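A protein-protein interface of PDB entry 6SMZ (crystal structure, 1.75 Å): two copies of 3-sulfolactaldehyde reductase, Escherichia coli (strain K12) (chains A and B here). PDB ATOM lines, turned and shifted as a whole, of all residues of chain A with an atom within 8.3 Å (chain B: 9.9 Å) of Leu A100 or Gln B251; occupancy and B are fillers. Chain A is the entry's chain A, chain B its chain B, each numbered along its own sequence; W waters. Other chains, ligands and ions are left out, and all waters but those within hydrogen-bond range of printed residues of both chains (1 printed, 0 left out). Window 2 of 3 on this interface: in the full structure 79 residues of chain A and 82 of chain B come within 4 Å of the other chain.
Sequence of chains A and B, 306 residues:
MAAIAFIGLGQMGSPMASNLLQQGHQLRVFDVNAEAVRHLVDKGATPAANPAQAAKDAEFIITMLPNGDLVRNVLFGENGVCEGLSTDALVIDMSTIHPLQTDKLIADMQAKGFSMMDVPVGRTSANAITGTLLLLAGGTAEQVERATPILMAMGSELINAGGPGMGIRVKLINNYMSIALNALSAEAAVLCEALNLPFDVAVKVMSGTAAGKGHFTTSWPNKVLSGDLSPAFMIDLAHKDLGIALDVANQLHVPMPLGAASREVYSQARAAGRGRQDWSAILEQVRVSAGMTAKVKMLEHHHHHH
The side-chain amide oxygen of Gln B251 sits at hydrogen-bond distance from a ring nitrogen (NE2) of His A98 (2.7 Å).
NE of Arg A169 sits at hydrogen-bond distance from O of Leu B195 (2.8 Å).
The backbone NH of Leu A100 is in hydrogen-bond range of a ring nitrogen (ND1) of His A98, 3.2 Å away.
NH1 of Arg A169 lies within salt-bridge range of OD2 of Asp A103.
O of Gly A165 lies within hydrogen-bond range of NH2 of Arg A169 (3.0 Å).
Ile B244 touches His A98.
Val B248 touches His A98 (CG2 to CE1, 3.5 Å).
Val B248 touches Pro A99 (CG2 to CD, 3.5 Å).
Leu A100 touches Gln B251.
CD1 of Leu A172 touches N of Ala B245 (3.9 Å).
Val B248 touches Leu A172.
Of chain B, only Gln B251 (3.7 Å) comes within 4 Å of Leu A100.
No residue of chain B comes within 4 Å of Asp A103.
Of the printed residues of chain B, Arg A169 touches Leu B195 (2.8 Å).
Leu B191 touches none of the printed residues of chain A.
Of the printed residues of chain A, Leu B195 touches Arg A169.
Printed residues of chain A within 4 Å of Ile B244: His A98.
Of the printed residues of chain A, Val B248 touches His A98 (3.5 Å), Pro A99 (3.5 Å) and Leu A172 (3.8 Å).
Gln B251 touches just these residues of chain A: His A98 and Leu A100.
Val B254 touches none of the printed residues of chain A.
The nearest printed residue of chain A that does not touch Leu B195 is Pro A99 (4.2 Å).
Of the 18 printed residues of chain B, 5 touch a printed residue of chain A.
Printed residues of chain B that touch a printed residue of chain A: Leu B195, Ile B244, Ala B245, Val B248 and Gln B251.
Hydrophobic or aromatic side chains of chain B that line the printed part of chain A: Leu B195, Ile B244, Ala B245 and Val B248.
Along chain B the printed residues that touch a printed residue of chain A span positions 195 to 251.
Hydrophobic or aromatic side chains of chain A that line the printed part of chain B: His A98, Pro A99, Leu A100 and Leu A172.
Among the printed residues, 8 pairs touch across the chains.
Among the printed residues, no Asp or Glu carboxylate lies within 4 Å of a Lys or Arg side-chain nitrogen of the other chain.
No position is printed for both chains.
Water W1 bridges NH1 of Arg A169 (3.0 Å) and O of Leu B195 (3.5 Å).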
ATOM      1  N   ARG A  72      -5.241 -24.974  31.629  1.00  0.00           N
ATOM      2  CA  ARG A  72      -6.157 -25.098  30.469  1.00  0.00           C
ATOM      3  C   ARG A  72      -7.261 -26.123  30.791  1.00  0.00           C
ATOM      4  O   ARG A  72      -8.431 -25.793  30.553  1.00  0.00           O
ATOM      5  CB  ARG A  72      -5.407 -25.469  29.187  1.00  0.00           C
ATOM      6  CG  ARG A  72      -6.348 -25.593  27.993  1.00  0.00           C
ATOM      7  CD  ARG A  72      -5.604 -25.512  26.666  1.00  0.00           C
ATOM      8  NE  ARG A  72      -5.189 -24.155  26.349  1.00  0.00           N
ATOM      9  CZ  ARG A  72      -5.949 -23.204  25.771  1.00  0.00           C
ATOM     10  NH1 ARG A  72      -5.427 -22.020  25.560  1.00  0.00           N
ATOM     11  NH2 ARG A  72      -7.214 -23.412  25.427  1.00  0.00           N
ATOM     12  N   ILE A  97       3.409 -20.477  34.637  1.00  0.00           N
ATOM     13  CA  ILE A  97       3.240 -21.285  33.410  1.00  0.00           C
ATOM     14  C   ILE A  97       3.942 -20.605  32.238  1.00  0.00           C
ATOM     15  O   ILE A  97       4.419 -19.475  32.409  1.00  0.00           O
ATOM     16  CB  ILE A  97       1.759 -21.552  33.122  1.00  0.00           C
ATOM     17  CG1 ILE A  97       1.003 -20.305  32.662  1.00  0.00           C
ATOM     18  CG2 ILE A  97       1.132 -22.245  34.311  1.00  0.00           C
ATOM     19  CD1 ILE A  97      -0.336 -20.577  32.033  1.00  0.00           C
ATOM     20  N   HIS A  98       3.972 -21.292  31.101  1.00  0.00           N
ATOM     21  CA  HIS A  98       4.593 -20.723  29.869  1.00  0.00           C
ATOM     22  C   HIS A  98       3.856 -19.448  29.483  1.00  0.00           C
ATOM     23  O   HIS A  98       2.635 -19.457  29.331  1.00  0.00           O
ATOM     24  CB  HIS A  98       4.565 -21.814  28.828  1.00  0.00           C
ATOM     25  CG  HIS A  98       5.333 -21.577  27.578  1.00  0.00           C
ATOM     26  ND1 HIS A  98       5.143 -20.468  26.765  1.00  0.00           N
ATOM     27  CD2 HIS A  98       6.214 -22.395  26.935  1.00  0.00           C
ATOM     28  CE1 HIS A  98       5.961 -20.570  25.714  1.00  0.00           C
ATOM     29  NE2 HIS A  98       6.615 -21.754  25.783  1.00  0.00           N
ATOM     30  N   PRO A  99       4.554 -18.316  29.303  1.00  0.00           N
ATOM     31  CA  PRO A  99       3.882 -17.036  29.058  1.00  0.00           C
ATOM     32  C   PRO A  99       3.078 -17.013  27.750  1.00  0.00           C
ATOM     33  O   PRO A  99       2.091 -16.291  27.675  1.00  0.00           O
ATOM     34  CB  PRO A  99       5.000 -15.992  29.008  1.00  0.00           C
ATOM     35  CG  PRO A  99       6.278 -16.788  28.842  1.00  0.00           C
ATOM     36  CD  PRO A  99       6.010 -18.179  29.392  1.00  0.00           C
ATOM     37  N   LEU A 100       3.464 -17.778  26.734  1.00  0.00           N
ATOM     38  CA  LEU A 100       2.657 -17.797  25.488  1.00  0.00           C
ATOM     39  C   LEU A 100       1.398 -18.652  25.684  1.00  0.00           C
ATOM     40  O   LEU A 100       0.389 -18.382  25.017  1.00  0.00           O
ATOM     41  CB  LEU A 100       3.520 -18.254  24.303  1.00  0.00           C
ATOM     42  CG  LEU A 100       4.849 -17.530  24.158  1.00  0.00           C
ATOM     43  CD1 LEU A 100       5.579 -18.045  22.915  1.00  0.00           C
ATOM     44  CD2 LEU A 100       4.663 -16.011  24.108  1.00  0.00           C
ATOM     45  N   GLN A 101       1.410 -19.616  26.615  1.00  0.00           N
ATOM     46  CA  GLN A 101       0.198 -20.362  27.031  1.00  0.00           C
ATOM     47  C   GLN A 101      -0.737 -19.390  27.762  1.00  0.00           C
ATOM     48  O   GLN A 101      -1.948 -19.424  27.535  1.00  0.00           O
ATOM     49  CB  GLN A 101       0.526 -21.530  27.965  1.00  0.00           C
ATOM     50  CG  GLN A 101       1.122 -22.779  27.312  1.00  0.00           C
ATOM     51  CD  GLN A 101       1.267 -23.877  28.365  1.00  0.00           C
ATOM     52  OE1 GLN A 101       1.904 -23.703  29.407  1.00  0.00           O
ATOM     53  NE2 GLN A 101       0.651 -25.024  28.130  1.00  0.00           N
ATOM     54  N   THR A 102      -0.202 -18.551  28.639  1.00  0.00           N
ATOM     55  CA  THR A 102      -0.989 -17.493  29.326  1.00  0.00           C
ATOM     56  C   THR A 102      -1.682 -16.629  28.268  1.00  0.00           C
ATOM     57  O   THR A 102      -2.899 -16.359  28.390  1.00  0.00           O
ATOM     58  CB  THR A 102      -0.112 -16.619  30.221  1.00  0.00           C
ATOM     59  OG1 THR A 102       0.437 -17.379  31.301  1.00  0.00           O
ATOM     60  CG2 THR A 102      -0.858 -15.437  30.790  1.00  0.00           C
ATOM     61  N   ASP A 103      -0.955 -16.163  27.259  1.00  0.00           N
ATOM     62  CA  ASP A 103      -1.546 -15.264  26.231  1.00  0.00           C
ATOM     63  C   ASP A 103      -2.703 -15.997  25.559  1.00  0.00           C
ATOM     64  O   ASP A 103      -3.765 -15.376  25.379  1.00  0.00           O
ATOM     65  CB  ASP A 103      -0.526 -14.892  25.157  1.00  0.00           C
ATOM     66  CG  ASP A 103       0.599 -14.004  25.618  1.00  0.00           C
ATOM     67  OD1 ASP A 103       0.517 -13.401  26.736  1.00  0.00           O
ATOM     68  OD2 ASP A 103       1.578 -13.937  24.859  1.00  0.00           O
ATOM     69  N   LYS A 104      -2.520 -17.274  25.208  1.00  0.00           N
ATOM     70  CA  LYS A 104      -3.553 -18.053  24.472  1.00  0.00           C
ATOM     71  C   LYS A 104      -4.754 -18.304  25.400  1.00  0.00           C
ATOM     72  O   LYS A 104      -5.918 -18.206  24.937  1.00  0.00           O
ATOM     73  CB  LYS A 104      -2.981 -19.358  23.913  1.00  0.00           C
ATOM     74  CG  LYS A 104      -3.858 -20.026  22.854  1.00  0.00           C
ATOM     75  CD  LYS A 104      -3.291 -21.328  22.316  1.00  0.00           C
ATOM     76  CE  LYS A 104      -4.236 -22.044  21.362  1.00  0.00           C
ATOM     77  NZ  LYS A 104      -5.525 -22.441  22.001  1.00  0.00           N
ATOM     78  N   LEU A 105      -4.526 -18.559  26.697  1.00  0.00           N
ATOM     79  CA  LEU A 105      -5.656 -18.741  27.649  1.00  0.00           C
ATOM     80  C   LEU A 105      -6.461 -17.443  27.723  1.00  0.00           C
ATOM     81  O   LEU A 105      -7.730 -17.486  27.637  1.00  0.00           O
ATOM     82  CB  LEU A 105      -5.109 -19.158  29.022  1.00  0.00           C
ATOM     83  CG  LEU A 105      -4.615 -20.595  29.101  1.00  0.00           C
ATOM     84  CD1 LEU A 105      -3.840 -20.828  30.371  1.00  0.00           C
ATOM     85  CD2 LEU A 105      -5.750 -21.593  28.984  1.00  0.00           C
ATOM     86  N   ILE A 106      -5.791 -16.306  27.891  1.00  0.00           N
ATOM     87  CA  ILE A 106      -6.454 -14.979  28.002  1.00  0.00           C
ATOM     88  C   ILE A 106      -7.268 -14.758  26.717  1.00  0.00           C
ATOM     89  O   ILE A 106      -8.450 -14.394  26.823  1.00  0.00           O
ATOM     90  CB  ILE A 106      -5.449 -13.851  28.304  1.00  0.00           C
ATOM     91  CG1 ILE A 106      -4.823 -14.029  29.686  1.00  0.00           C
ATOM     92  CG2 ILE A 106      -6.083 -12.479  28.170  1.00  0.00           C
ATOM     93  CD1 ILE A 106      -3.779 -13.007  30.077  1.00  0.00           C
ATOM     94  N   ALA A 107      -6.688 -15.016  25.554  1.00  0.00           N
ATOM     95  CA  ALA A 107      -7.346 -14.761  24.252  1.00  0.00           C
ATOM     96  C   ALA A 107      -8.548 -15.698  24.094  1.00  0.00           C
ATOM     97  O   ALA A 107      -9.621 -15.233  23.630  1.00  0.00           O
ATOM     98  CB  ALA A 107      -6.372 -14.944  23.106  1.00  0.00           C
ATOM     99  N   GLY A 165      -0.484 -10.524  30.396  1.00  0.00           N
ATOM    100  CA  GLY A 165       0.673 -11.401  30.122  1.00  0.00           C
ATOM    101  C   GLY A 165       2.000 -10.839  30.614  1.00  0.00           C
ATOM    102  O   GLY A 165       3.005 -11.575  30.537  1.00  0.00           O
ATOM    103  N   ILE A 168       3.340 -12.740  34.102  1.00  0.00           N
ATOM    104  CA  ILE A 168       4.004 -14.056  33.896  1.00  0.00           C
ATOM    105  C   ILE A 168       5.336 -13.801  33.198  1.00  0.00           C
ATOM    106  O   ILE A 168       6.308 -14.482  33.530  1.00  0.00           O
ATOM    107  CB  ILE A 168       3.101 -15.065  33.188  1.00  0.00           C
ATOM    108  CG1 ILE A 168       3.772 -16.433  33.133  1.00  0.00           C
ATOM    109  CG2 ILE A 168       2.671 -14.598  31.810  1.00  0.00           C
ATOM    110  CD1 ILE A 168       4.178 -17.021  34.462  1.00  0.00           C
ATOM    111  N   ARG A 169       5.422 -12.805  32.318  1.00  0.00           N
ATOM    112  CA  ARG A 169       6.718 -12.507  31.645  1.00  0.00           C
ATOM    113  C   ARG A 169       7.736 -12.052  32.688  1.00  0.00           C
ATOM    114  O   ARG A 169       8.871 -12.583  32.679  1.00  0.00           O
ATOM    115  CB  ARG A 169       6.501 -11.484  30.528  1.00  0.00           C
ATOM    116  CG  ARG A 169       5.901 -12.051  29.272  1.00  0.00           C
ATOM    117  CD  ARG A 169       5.358 -10.936  28.394  1.00  0.00           C
ATOM    118  NE  ARG A 169       5.018 -11.416  27.086  1.00  0.00           N
ATOM    119  CZ  ARG A 169       3.993 -12.174  26.763  1.00  0.00           C
ATOM    120  NH1 ARG A 169       3.861 -12.562  25.515  1.00  0.00           N
ATOM    121  NH2 ARG A 169       3.126 -12.596  27.676  1.00  0.00           N
ATOM    122  N   LEU A 172       8.901 -14.908  34.845  1.00  0.00           N
ATOM    123  CA  LEU A 172       9.794 -15.834  34.106  1.00  0.00           C
ATOM    124  C   LEU A 172      11.199 -15.223  34.002  1.00  0.00           C
ATOM    125  O   LEU A 172      12.178 -15.960  34.238  1.00  0.00           O
ATOM    126  CB  LEU A 172       9.202 -16.146  32.737  1.00  0.00           C
ATOM    127  CG  LEU A 172      10.038 -17.155  31.947  1.00  0.00           C
ATOM    128  CD1 LEU A 172      10.106 -18.493  32.663  1.00  0.00           C
ATOM    129  CD2 LEU A 172       9.545 -17.302  30.542  1.00  0.00           C
ATOM    130  N   LEU B 191      15.912 -12.136  26.381  1.00  0.00           N
ATOM    131  CA  LEU B 191      14.647 -12.883  26.484  1.00  0.00           C
ATOM    132  C   LEU B 191      13.529 -11.912  26.893  1.00  0.00           C
ATOM    133  O   LEU B 191      12.431 -11.994  26.323  1.00  0.00           O
ATOM    134  CB  LEU B 191      14.803 -14.016  27.484  1.00  0.00           C
ATOM    135  CG  LEU B 191      13.581 -14.946  27.568  1.00  0.00           C
ATOM    136  CD1 LEU B 191      13.297 -15.591  26.261  1.00  0.00           C
ATOM    137  CD2 LEU B 191      13.789 -15.985  28.643  1.00  0.00           C
ATOM    138  N   ALA B 194      12.548  -9.979  23.821  1.00  0.00           N
ATOM    139  CA  ALA B 194      11.849 -10.839  22.862  1.00  0.00           C
ATOM    140  C   ALA B 194      10.393 -11.043  23.308  1.00  0.00           C
ATOM    141  O   ALA B 194       9.559 -11.322  22.435  1.00  0.00           O
ATOM    142  CB  ALA B 194      12.565 -12.158  22.741  1.00  0.00           C
ATOM    143  N   LEU B 195      10.155 -11.022  24.613  1.00  0.00           N
ATOM    144  CA  LEU B 195       8.771 -11.190  25.184  1.00  0.00           C
ATOM    145  C   LEU B 195       8.020  -9.841  25.201  1.00  0.00           C
ATOM    146  O   LEU B 195       6.864  -9.836  25.653  1.00  0.00           O
ATOM    147  CB  LEU B 195       8.924 -11.775  26.589  1.00  0.00           C
ATOM    148  CG  LEU B 195       9.165 -13.278  26.625  1.00  0.00           C
ATOM    149  CD1 LEU B 195       9.561 -13.704  28.028  1.00  0.00           C
ATOM    150  CD2 LEU B 195       7.900 -13.993  26.193  1.00  0.00           C
ATOM    151  N   ASN B 196       8.647  -8.749  24.767  1.00  0.00           N
ATOM    152  CA  ASN B 196       8.014  -7.398  24.748  1.00  0.00           C
ATOM    153  C   ASN B 196       7.703  -6.945  26.176  1.00  0.00           C
ATOM    154  O   ASN B 196       6.713  -6.196  26.356  1.00  0.00           O
ATOM    155  CB  ASN B 196       6.761  -7.363  23.878  1.00  0.00           C
ATOM    156  N   GLY B 243      13.309 -25.000  32.564  1.00  0.00           N
ATOM    157  CA  GLY B 243      12.752 -25.661  31.376  1.00  0.00           C
ATOM    158  C   GLY B 243      11.777 -24.765  30.624  1.00  0.00           C
ATOM    159  O   GLY B 243      11.871 -24.662  29.391  1.00  0.00           O
ATOM    160  N   ILE B 244      10.857 -24.105  31.319  1.00  0.00           N
ATOM    161  CA  ILE B 244       9.921 -23.158  30.678  1.00  0.00           C
ATOM    162  C   ILE B 244      10.711 -22.020  30.037  1.00  0.00           C
ATOM    163  O   ILE B 244      10.389 -21.662  28.881  1.00  0.00           O
ATOM    164  CB  ILE B 244       8.873 -22.618  31.672  1.00  0.00           C
ATOM    165  CG1 ILE B 244       8.063 -23.763  32.298  1.00  0.00           C
ATOM    166  CG2 ILE B 244       8.014 -21.539  31.016  1.00  0.00           C
ATOM    167  CD1 ILE B 244       7.208 -23.251  33.462  1.00  0.00           C
ATOM    168  N   ALA B 245      11.674 -21.444  30.742  1.00  0.00           N
ATOM    169  CA  ALA B 245      12.480 -20.322  30.204  1.00  0.00           C
ATOM    170  C   ALA B 245      13.151 -20.787  28.900  1.00  0.00           C
ATOM    171  O   ALA B 245      13.133 -20.029  27.926  1.00  0.00           O
ATOM    172  CB  ALA B 245      13.455 -19.833  31.229  1.00  0.00           C
ATOM    173  N   LEU B 246      13.725 -21.988  28.880  1.00  0.00           N
ATOM    174  CA  LEU B 246      14.425 -22.487  27.661  1.00  0.00           C
ATOM    175  C   LEU B 246      13.422 -22.798  26.560  1.00  0.00           C
ATOM    176  O   LEU B 246      13.737 -22.592  25.388  1.00  0.00           O
ATOM    177  CB  LEU B 246      15.276 -23.694  28.050  1.00  0.00           C
ATOM    178  CG  LEU B 246      16.539 -23.288  28.807  1.00  0.00           C
ATOM    179  CD1 LEU B 246      17.147 -24.466  29.559  1.00  0.00           C
ATOM    180  CD2 LEU B 246      17.554 -22.689  27.840  1.00  0.00           C
ATOM    181  N   ASP B 247      12.224 -23.306  26.897  1.00  0.00           N
ATOM    182  CA  ASP B 247      11.164 -23.526  25.886  1.00  0.00           C
ATOM    183  C   ASP B 247      10.830 -22.186  25.217  1.00  0.00           C
ATOM    184  O   ASP B 247      10.766 -22.127  23.958  1.00  0.00           O
ATOM    185  CB  ASP B 247       9.905 -24.136  26.514  1.00  0.00           C
ATOM    186  CG  ASP B 247      10.013 -25.555  27.041  1.00  0.00           C
ATOM    187  OD1 ASP B 247      10.834 -26.343  26.494  1.00  0.00           O
ATOM    188  OD2 ASP B 247       9.200 -25.889  27.989  1.00  0.00           O
ATOM    189  N   VAL B 248      10.622 -21.146  26.007  1.00  0.00           N
ATOM    190  CA  VAL B 248      10.262 -19.797  25.484  1.00  0.00           C
ATOM    191  C   VAL B 248      11.411 -19.272  24.613  1.00  0.00           C
ATOM    192  O   VAL B 248      11.159 -18.842  23.494  1.00  0.00           O
ATOM    193  CB  VAL B 248       9.929 -18.819  26.607  1.00  0.00           C
ATOM    194  CG1 VAL B 248       9.716 -17.431  26.056  1.00  0.00           C
ATOM    195  CG2 VAL B 248       8.704 -19.292  27.397  1.00  0.00           C
ATOM    196  N   ALA B 249      12.618 -19.302  25.129  1.00  0.00           N
ATOM    197  CA  ALA B 249      13.818 -18.822  24.384  1.00  0.00           C
ATOM    198  C   ALA B 249      13.912 -19.535  23.047  1.00  0.00           C
ATOM    199  O   ALA B 249      14.210 -18.888  22.011  1.00  0.00           O
ATOM    200  CB  ALA B 249      15.058 -19.001  25.242  1.00  0.00           C
ATOM    201  N   ASN B 250      13.730 -20.857  23.018  1.00  0.00           N
ATOM    202  CA  ASN B 250      13.860 -21.640  21.764  1.00  0.00           C
ATOM    203  C   ASN B 250      12.708 -21.327  20.829  1.00  0.00           C
ATOM    204  O   ASN B 250      12.915 -21.293  19.614  1.00  0.00           O
ATOM    205  CB  ASN B 250      14.098 -23.115  22.077  1.00  0.00           C
ATOM    206  CG  ASN B 250      15.580 -23.324  22.326  1.00  0.00           C
ATOM    207  OD1 ASN B 250      16.340 -23.435  21.359  1.00  0.00           O
ATOM    208  ND2 ASN B 250      16.002 -23.352  23.583  1.00  0.00           N
ATOM    209  N   GLN B 251      11.516 -21.044  21.365  1.00  0.00           N
ATOM    210  CA  GLN B 251      10.408 -20.640  20.475  1.00  0.00           C
ATOM    211  C   GLN B 251      10.715 -19.260  19.882  1.00  0.00           C
ATOM    212  O   GLN B 251      10.278 -18.998  18.721  1.00  0.00           O
ATOM    213  CB  GLN B 251       9.098 -20.628  21.289  1.00  0.00           C
ATOM    214  CG  GLN B 251       8.341 -21.941  21.244  1.00  0.00           C
ATOM    215  CD  GLN B 251       7.005 -21.688  21.913  1.00  0.00           C
ATOM    216  OE1 GLN B 251       6.981 -21.482  23.103  1.00  0.00           O
ATOM    217  NE2 GLN B 251       5.966 -21.451  21.126  1.00  0.00           N
ATOM    218  N   LEU B 252      11.395 -18.389  20.614  1.00  0.00           N
ATOM    219  CA  LEU B 252      11.617 -16.968  20.200  1.00  0.00           C
ATOM    220  C   LEU B 252      13.022 -16.796  19.573  1.00  0.00           C
ATOM    221  O   LEU B 252      13.409 -15.650  19.323  1.00  0.00           O
ATOM    222  CB  LEU B 252      11.443 -16.071  21.419  1.00  0.00           C
ATOM    223  CG  LEU B 252      10.045 -16.081  22.050  1.00  0.00           C
ATOM    224  CD1 LEU B 252       9.962 -15.072  23.167  1.00  0.00           C
ATOM    225  CD2 LEU B 252       8.969 -15.820  21.031  1.00  0.00           C
ATOM    226  N   HIS B 253      13.753 -17.885  19.338  1.00  0.00           N
ATOM    227  CA  HIS B 253      15.174 -17.884  18.876  1.00  0.00           C
ATOM    228  C   HIS B 253      16.030 -16.840  19.609  1.00  0.00           C
ATOM    229  O   HIS B 253      16.800 -16.072  18.970  1.00  0.00           O
ATOM    230  CB  HIS B 253      15.251 -17.824  17.347  1.00  0.00           C
ATOM    231  CG  HIS B 253      14.609 -16.644  16.704  1.00  0.00           C
ATOM    232  ND1 HIS B 253      15.107 -15.348  16.832  1.00  0.00           N
ATOM    233  CD2 HIS B 253      13.582 -16.570  15.831  1.00  0.00           C
ATOM    234  CE1 HIS B 253      14.344 -14.518  16.111  1.00  0.00           C
ATOM    235  NE2 HIS B 253      13.397 -15.230  15.534  1.00  0.00           N
ATOM    236  N   VAL B 254      15.987 -16.882  20.937  1.00  0.00           N
ATOM    237  CA  VAL B 254      16.935 -16.182  21.820  1.00  0.00           C
ATOM    238  C   VAL B 254      17.934 -17.226  22.303  1.00  0.00           C
ATOM    239  O   VAL B 254      17.600 -18.060  23.138  1.00  0.00           O
ATOM    240  CB  VAL B 254      16.250 -15.521  23.014  1.00  0.00           C
ATOM    241  CG1 VAL B 254      17.271 -14.852  23.922  1.00  0.00           C
ATOM    242  CG2 VAL B 254      15.188 -14.534  22.541  1.00  0.00           C
ATOM    243  N   PRO B 255      19.174 -17.252  21.776  1.00  0.00           N
ATOM    244  CA  PRO B 255      20.151 -18.239  22.213  1.00  0.00           C
ATOM    245  C   PRO B 255      20.534 -18.036  23.674  1.00  0.00           C
ATOM    246  O   PRO B 255      20.876 -16.916  24.066  1.00  0.00           O
ATOM    247  CB  PRO B 255      21.350 -18.046  21.277  1.00  0.00           C
ATOM    248  CG  PRO B 255      20.713 -17.388  20.053  1.00  0.00           C
ATOM    249  CD  PRO B 255      19.697 -16.438  20.668  1.00  0.00           C
ATOM    250  N   MET B 256      20.445 -19.102  24.475  1.00  0.00           N
ATOM    251  CA  MET B 256      20.742 -19.001  25.919  1.00  0.00           C
ATOM    252  C   MET B 256      21.681 -20.133  26.323  1.00  0.00           C
ATOM    253  O   MET B 256      21.312 -21.040  27.051  1.00  0.00           O
ATOM    254  CB  MET B 256      19.476 -19.011  26.794  1.00  0.00           C
ATOM    255  CG  MET B 256      18.524 -17.879  26.409  1.00  0.00           C
ATOM    256  SD  MET B 256      17.480 -17.295  27.761  1.00  0.00           S
ATOM    257  CE  MET B 256      16.848 -18.849  28.399  1.00  0.00           C
HETATM  258  O   HOH W   1       4.879 -11.138  23.099  1.00  0.00           O
